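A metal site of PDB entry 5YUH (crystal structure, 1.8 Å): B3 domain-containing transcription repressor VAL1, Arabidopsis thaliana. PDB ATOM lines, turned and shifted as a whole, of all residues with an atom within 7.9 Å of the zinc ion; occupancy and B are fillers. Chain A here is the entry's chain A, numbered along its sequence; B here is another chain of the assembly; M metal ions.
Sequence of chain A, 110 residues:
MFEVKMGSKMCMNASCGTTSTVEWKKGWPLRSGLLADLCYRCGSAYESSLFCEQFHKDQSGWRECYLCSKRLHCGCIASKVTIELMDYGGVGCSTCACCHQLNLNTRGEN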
ATOM      1  N   TRP A  28      29.608  15.307 -18.066  1.00  0.00           N
ATOM      2  CA  TRP A  28      28.325  15.843 -18.506  1.00  0.00           C
ATOM      3  C   TRP A  28      28.526  17.022 -19.461  1.00  0.00           C
ATOM      4  O   TRP A  28      29.619  17.602 -19.536  1.00  0.00           O
ATOM      5  CB  TRP A  28      27.512  16.276 -17.289  1.00  0.00           C
ATOM      6  CG  TRP A  28      28.307  17.135 -16.364  1.00  0.00           C
ATOM      7  CD1 TRP A  28      28.430  18.498 -16.403  1.00  0.00           C
ATOM      8  CD2 TRP A  28      29.118  16.696 -15.264  1.00  0.00           C
ATOM      9  NE1 TRP A  28      29.257  18.931 -15.386  1.00  0.00           N
ATOM     10  CE2 TRP A  28      29.687  17.850 -14.676  1.00  0.00           C
ATOM     11  CE3 TRP A  28      29.395  15.440 -14.702  1.00  0.00           C
ATOM     12  CZ2 TRP A  28      30.540  17.782 -13.567  1.00  0.00           C
ATOM     13  CZ3 TRP A  28      30.248  15.373 -13.592  1.00  0.00           C
ATOM     14  CH2 TRP A  28      30.790  16.536 -13.039  1.00  0.00           C
ATOM     15  N   PHE A  51      27.469   8.362 -10.873  1.00  0.00           N
ATOM     16  CA  PHE A  51      28.184   9.515 -10.363  1.00  0.00           C
ATOM     17  C   PHE A  51      27.487  10.110  -9.135  1.00  0.00           C
ATOM     18  O   PHE A  51      28.101  10.275  -8.068  1.00  0.00           O
ATOM     19  CB  PHE A  51      28.347  10.553 -11.470  1.00  0.00           C
ATOM     20  CG  PHE A  51      29.158  11.726 -11.069  1.00  0.00           C
ATOM     21  CD1 PHE A  51      28.566  12.840 -10.506  1.00  0.00           C
ATOM     22  CD2 PHE A  51      30.542  11.721 -11.258  1.00  0.00           C
ATOM     23  CE1 PHE A  51      29.330  13.930 -10.122  1.00  0.00           C
ATOM     24  CE2 PHE A  51      31.315  12.789 -10.894  1.00  0.00           C
ATOM     25  CZ  PHE A  51      30.717  13.908 -10.325  1.00  0.00           C
ATOM     26  N   CYS A  52      26.202  10.451  -9.265  1.00  0.00           N
ATOM     27  CA  CYS A  52      25.557  11.122  -8.142  1.00  0.00           C
ATOM     28  C   CYS A  52      25.369  10.205  -6.939  1.00  0.00           C
ATOM     29  O   CYS A  52      25.460  10.674  -5.801  1.00  0.00           O
ATOM     30  CB  CYS A  52      24.206  11.689  -8.560  1.00  0.00           C
ATOM     31  SG  CYS A  52      24.458  13.043  -9.677  1.00  0.00           S
ATOM     32  N   GLU A  53      25.110   8.922  -7.167  1.00  0.00           N
ATOM     33  CA  GLU A  53      25.059   7.987  -6.052  1.00  0.00           C
ATOM     34  C   GLU A  53      26.377   7.975  -5.286  1.00  0.00           C
ATOM     35  O   GLU A  53      26.399   7.916  -4.054  1.00  0.00           O
ATOM     36  CB  GLU A  53      24.707   6.582  -6.552  1.00  0.00           C
ATOM     37  CG  GLU A  53      23.246   6.406  -6.978  1.00  0.00           C
ATOM     38  CD  GLU A  53      22.926   6.867  -8.417  1.00  0.00           C
ATOM     39  OE1 GLU A  53      23.800   7.480  -9.109  1.00  0.00           O
ATOM     40  OE2 GLU A  53      21.774   6.599  -8.866  1.00  0.00           O
ATOM     41  N   PHE A  55      28.935  10.387  -5.259  1.00  0.00           N
ATOM     42  CA  PHE A  55      29.529  11.645  -4.810  1.00  0.00           C
ATOM     43  C   PHE A  55      28.555  12.645  -4.217  1.00  0.00           C
ATOM     44  O   PHE A  55      28.993  13.558  -3.512  1.00  0.00           O
ATOM     45  CB  PHE A  55      30.263  12.329  -5.964  1.00  0.00           C
ATOM     46  CG  PHE A  55      31.441  11.545  -6.499  1.00  0.00           C
ATOM     47  CD1 PHE A  55      32.599  11.412  -5.738  1.00  0.00           C
ATOM     48  CD2 PHE A  55      31.384  10.950  -7.753  1.00  0.00           C
ATOM     49  CE1 PHE A  55      33.678  10.693  -6.229  1.00  0.00           C
ATOM     50  CE2 PHE A  55      32.463  10.231  -8.244  1.00  0.00           C
ATOM     51  CZ  PHE A  55      33.621  10.098  -7.484  1.00  0.00           C
ATOM     52  N   HIS A  56      27.250  12.523  -4.481  1.00  0.00           N
ATOM     53  CA  HIS A  56      26.305  13.557  -4.093  1.00  0.00           C
ATOM     54  C   HIS A  56      25.303  13.064  -3.052  1.00  0.00           C
ATOM     55  O   HIS A  56      24.294  13.731  -2.828  1.00  0.00           O
ATOM     56  CB  HIS A  56      25.592  14.121  -5.331  1.00  0.00           C
ATOM     57  CG  HIS A  56      26.495  14.900  -6.234  1.00  0.00           C
ATOM     58  ND1 HIS A  56      26.076  15.412  -7.447  1.00  0.00           N
ATOM     59  CD2 HIS A  56      27.798  15.259  -6.107  1.00  0.00           C
ATOM     60  CE1 HIS A  56      27.092  16.043  -8.023  1.00  0.00           C
ATOM     61  NE2 HIS A  56      28.134  15.980  -7.221  1.00  0.00           N
ATOM     62  N   LYS A  57      25.592  11.930  -2.393  1.00  0.00           N
ATOM     63  CA  LYS A  57      24.676  11.330  -1.421  1.00  0.00           C
ATOM     64  C   LYS A  57      24.150  12.334  -0.396  1.00  0.00           C
ATOM     65  O   LYS A  57      22.960  12.353  -0.073  1.00  0.00           O
ATOM     66  CB  LYS A  57      25.373  10.196  -0.677  1.00  0.00           C
ATOM     67  CG  LYS A  57      25.359   8.821  -1.302  1.00  0.00           C
ATOM     68  CD  LYS A  57      26.347   7.901  -0.533  1.00  0.00           C
ATOM     69  CE  LYS A  57      26.379   6.482  -1.090  1.00  0.00           C
ATOM     70  NZ  LYS A  57      27.495   6.241  -2.072  1.00  0.00           N
ATOM     71  N   GLN A  59      23.963  15.578  -0.534  1.00  0.00           N
ATOM     72  CA  GLN A  59      23.528  16.887  -1.029  1.00  0.00           C
ATOM     73  C   GLN A  59      22.013  16.988  -1.069  1.00  0.00           C
ATOM     74  O   GLN A  59      21.284  15.989  -1.041  1.00  0.00           O
ATOM     75  CB  GLN A  59      24.094  17.158  -2.420  1.00  0.00           C
ATOM     76  CG  GLN A  59      25.596  17.286  -2.440  1.00  0.00           C
ATOM     77  CD  GLN A  59      26.120  17.730  -3.783  1.00  0.00           C
ATOM     78  OE1 GLN A  59      25.352  18.063  -4.693  1.00  0.00           O
ATOM     79  NE2 GLN A  59      27.445  17.752  -3.919  1.00  0.00           N
ATOM     80  N   SER A  60      21.535  18.228  -1.161  1.00  0.00           N
ATOM     81  CA  SER A  60      20.117  18.443  -1.348  1.00  0.00           C
ATOM     82  C   SER A  60      19.742  18.105  -2.791  1.00  0.00           C
ATOM     83  O   SER A  60      20.589  17.981  -3.669  1.00  0.00           O
ATOM     84  CB  SER A  60      19.753  19.887  -1.025  1.00  0.00           C
ATOM     85  OG  SER A  60      20.533  20.744  -1.816  1.00  0.00           O
ATOM     86  N   TRP A  62      17.618  15.418  -3.927  1.00  0.00           N
ATOM     87  CA  TRP A  62      17.190  14.075  -4.291  1.00  0.00           C
ATOM     88  C   TRP A  62      15.672  13.941  -4.232  1.00  0.00           C
ATOM     89  O   TRP A  62      15.033  14.311  -3.238  1.00  0.00           O
ATOM     90  CB  TRP A  62      17.838  13.027  -3.391  1.00  0.00           C
ATOM     91  CG  TRP A  62      19.307  12.870  -3.541  1.00  0.00           C
ATOM     92  CD1 TRP A  62      20.291  13.515  -2.838  1.00  0.00           C
ATOM     93  CD2 TRP A  62      19.977  11.977  -4.435  1.00  0.00           C
ATOM     94  NE1 TRP A  62      21.528  13.081  -3.245  1.00  0.00           N
ATOM     95  CE2 TRP A  62      21.356  12.136  -4.235  1.00  0.00           C
ATOM     96  CE3 TRP A  62      19.540  11.068  -5.407  1.00  0.00           C
ATOM     97  CZ2 TRP A  62      22.315  11.417  -4.953  1.00  0.00           C
ATOM     98  CZ3 TRP A  62      20.489  10.343  -6.113  1.00  0.00           C
ATOM     99  CH2 TRP A  62      21.858  10.526  -5.893  1.00  0.00           C
ATOM    100  N   LEU A  72      16.762  10.012  -7.575  1.00  0.00           N
ATOM    101  CA  LEU A  72      17.225  10.836  -8.698  1.00  0.00           C
ATOM    102  C   LEU A  72      17.732  12.160  -8.145  1.00  0.00           C
ATOM    103  O   LEU A  72      17.010  12.836  -7.413  1.00  0.00           O
ATOM    104  CB  LEU A  72      16.087  11.101  -9.679  1.00  0.00           C
ATOM    105  CG  LEU A  72      15.461   9.853 -10.315  1.00  0.00           C
ATOM    106  CD1 LEU A  72      14.210  10.259 -11.103  1.00  0.00           C
ATOM    107  CD2 LEU A  72      16.511   9.205 -11.181  1.00  0.00           C
ATOM    108  N   HIS A  73      18.966  12.535  -8.494  1.00  0.00           N
ATOM    109  CA  HIS A  73      19.557  13.753  -7.945  1.00  0.00           C
ATOM    110  C   HIS A  73      19.155  14.927  -8.830  1.00  0.00           C
ATOM    111  O   HIS A  73      19.717  15.119  -9.904  1.00  0.00           O
ATOM    112  CB  HIS A  73      21.069  13.634  -7.825  1.00  0.00           C
ATOM    113  CG  HIS A  73      21.655  14.739  -7.009  1.00  0.00           C
ATOM    114  ND1 HIS A  73      22.928  15.220  -7.207  1.00  0.00           N
ATOM    115  CD2 HIS A  73      21.122  15.459  -5.993  1.00  0.00           C
ATOM    116  CE1 HIS A  73      23.153  16.201  -6.351  1.00  0.00           C
ATOM    117  NE2 HIS A  73      22.078  16.367  -5.592  1.00  0.00           N
ATOM    118  N   CYS A  74      18.181  15.701  -8.374  1.00  0.00           N
ATOM    119  CA  CYS A  74      17.678  16.813  -9.165  1.00  0.00           C
ATOM    120  C   CYS A  74      18.496  18.073  -8.871  1.00  0.00           C
ATOM    121  O   CYS A  74      19.279  18.151  -7.914  1.00  0.00           O
ATOM    122  CB  CYS A  74      16.194  17.040  -8.896  1.00  0.00           C
ATOM    123  SG  CYS A  74      15.123  15.557  -9.170  1.00  0.00           S
ATOM    124  N   GLY A  75      18.279  19.080  -9.710  1.00  0.00           N
ATOM    125  CA  GLY A  75      19.087  20.274  -9.614  1.00  0.00           C
ATOM    126  C   GLY A  75      20.555  20.007  -9.778  1.00  0.00           C
ATOM    127  O   GLY A  75      21.374  20.708  -9.181  1.00  0.00           O
ATOM    128  N   CYS A  76      20.935  19.016 -10.588  1.00  0.00           N
ATOM    129  CA  CYS A  76      22.323  18.590 -10.697  1.00  0.00           C
ATOM    130  C   CYS A  76      22.635  18.285 -12.156  1.00  0.00           C
ATOM    131  O   CYS A  76      22.018  17.390 -12.747  1.00  0.00           O
ATOM    132  CB  CYS A  76      22.627  17.355  -9.847  1.00  0.00           C
ATOM    133  SG  CYS A  76      24.348  16.844  -9.995  1.00  0.00           S
ATOM    134  N   ILE A  77      23.631  18.996 -12.692  1.00  0.00           N
ATOM    135  CA  ILE A  77      23.990  18.826 -14.084  1.00  0.00           C
ATOM    136  C   ILE A  77      24.439  17.397 -14.374  1.00  0.00           C
ATOM    137  O   ILE A  77      24.137  16.851 -15.441  1.00  0.00           O
ATOM    138  CB  ILE A  77      25.048  19.888 -14.441  1.00  0.00           C
ATOM    139  CG1 ILE A  77      25.234  19.999 -15.941  1.00  0.00           C
ATOM    140  CG2 ILE A  77      26.377  19.611 -13.717  1.00  0.00           C
ATOM    141  CD1 ILE A  77      26.031  21.235 -16.323  1.00  0.00           C
ATOM    142  N   ALA A  78      25.084  16.743 -13.395  1.00  0.00           N
ATOM    143  CA  ALA A  78      25.638  15.405 -13.605  1.00  0.00           C
ATOM    144  C   ALA A  78      24.565  14.344 -13.858  1.00  0.00           C
ATOM    145  O   ALA A  78      24.886  13.283 -14.427  1.00  0.00           O
ATOM    146  CB  ALA A  78      26.480  14.968 -12.412  1.00  0.00           C
ATOM    147  N   SER A  79      23.330  14.570 -13.421  1.00  0.00           N
ATOM    148  CA  SER A  79      22.236  13.641 -13.635  1.00  0.00           C
ATOM    149  C   SER A  79      21.202  14.165 -14.608  1.00  0.00           C
ATOM    150  O   SER A  79      20.191  13.494 -14.833  1.00  0.00           O
ATOM    151  CB  SER A  79      21.545  13.301 -12.313  1.00  0.00           C
ATOM    152  OG  SER A  79      22.261  12.300 -11.608  1.00  0.00           O
ATOM    153  N   LYS A  80      21.436  15.366 -15.187  1.00  0.00           N
ATOM    154  CA  LYS A  80      20.372  16.035 -15.943  1.00  0.00           C
ATOM    155  C   LYS A  80      19.827  15.155 -17.060  1.00  0.00           C
ATOM    156  O   LYS A  80      18.612  15.043 -17.234  1.00  0.00           O
ATOM    157  CB  LYS A  80      20.899  17.340 -16.526  1.00  0.00           C
ATOM    158  CG  LYS A  80      19.819  18.135 -17.248  1.00  0.00           C
ATOM    159  CD  LYS A  80      20.410  19.402 -17.869  1.00  0.00           C
ATOM    160  CE  LYS A  80      19.360  20.198 -18.614  1.00  0.00           C
ATOM    161  NZ  LYS A  80      19.986  21.210 -19.495  1.00  0.00           N
ATOM    162  N   ILE A  83      17.079  12.345 -16.037  1.00  0.00           N
ATOM    163  CA  ILE A  83      15.901  12.703 -15.257  1.00  0.00           C
ATOM    164  C   ILE A  83      14.901  13.426 -16.150  1.00  0.00           C
ATOM    165  O   ILE A  83      15.259  14.417 -16.783  1.00  0.00           O
ATOM    166  CB  ILE A  83      16.281  13.589 -14.050  1.00  0.00           C
ATOM    167  CG1 ILE A  83      17.104  12.768 -13.049  1.00  0.00           C
ATOM    168  CG2 ILE A  83      15.043  14.238 -13.463  1.00  0.00           C
ATOM    169  CD1 ILE A  83      17.742  13.593 -11.926  1.00  0.00           C
ATOM    170  N   ARG B  63      16.558  22.853  -3.242  1.00  0.00           N
ATOM    171  CA  ARG B  63      17.942  23.192  -3.004  1.00  0.00           C
ATOM    172  C   ARG B  63      18.034  24.700  -2.760  1.00  0.00           C
ATOM    173  O   ARG B  63      17.044  25.423  -2.836  1.00  0.00           O
ATOM    174  CB  ARG B  63      18.831  22.797  -4.170  1.00  0.00           C
ATOM    175  CG  ARG B  63      18.627  21.392  -4.697  1.00  0.00           C
ATOM    176  CD  ARG B  63      19.744  21.018  -5.620  1.00  0.00           C
ATOM    177  NE  ARG B  63      20.960  20.824  -4.847  1.00  0.00           N
ATOM    178  CZ  ARG B  63      22.094  20.327  -5.327  1.00  0.00           C
ATOM    179  NH1 ARG B  63      22.182  19.945  -6.594  1.00  0.00           N
ATOM    180  NH2 ARG B  63      23.133  20.201  -4.518  1.00  0.00           N
ATOM    181  N   GLY B  89      27.935  21.443 -10.351  1.00  0.00           N
ATOM    182  CA  GLY B  89      26.993  21.015  -9.348  1.00  0.00           C
ATOM    183  C   GLY B  89      26.224  22.180  -8.750  1.00  0.00           C
ATOM    184  O   GLY B  89      26.649  23.340  -8.798  1.00  0.00           O
ATOM    185  N   GLY B  90      25.083  21.856  -8.178  1.00  0.00           N
ATOM    186  CA  GLY B  90      24.274  22.858  -7.515  1.00  0.00           C
ATOM    187  C   GLY B  90      23.518  23.693  -8.517  1.00  0.00           C
ATOM    188  O   GLY B  90      23.597  23.507  -9.743  1.00  0.00           O
HETATM  189 ZN    ZN M   1      24.354  15.030  -8.506  1.00  0.00          ZN
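O of Ser 60 sits at hydrogen-bond distance from NE2 of His 73, 2.9 Å away.
The backbone carbonyl oxygen (O) of His 56 is in hydrogen-bond range of the indole nitrogen (NE1) of Trp 62 (2.9 Å).
The backbone NH of Ala 78 sits close to the side-chain sulfur of Cys 76 (3.5 Å).
SG of Cys 52 lies close to OG of Ser 79 (3.0 Å).
Within 4 Å of the zinc ion: Cys 52, His 56, His 73 and Cys 76.
The nearest printed residue that does not touch the zinc ion is Ala 78 (4.4 Å).
ND1 of His 73 binds the zinc ion, 1.9 Å away.
ND1 of His 56 is bound to the zinc ion (2.1 Å).
The zinc ion is bound by the side-chain sulfur (SG) of Cys 52 (2.3 Å).
The zinc ion is bound by SG of Cys 76.
The zinc ion has four donor atoms within binding distance.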
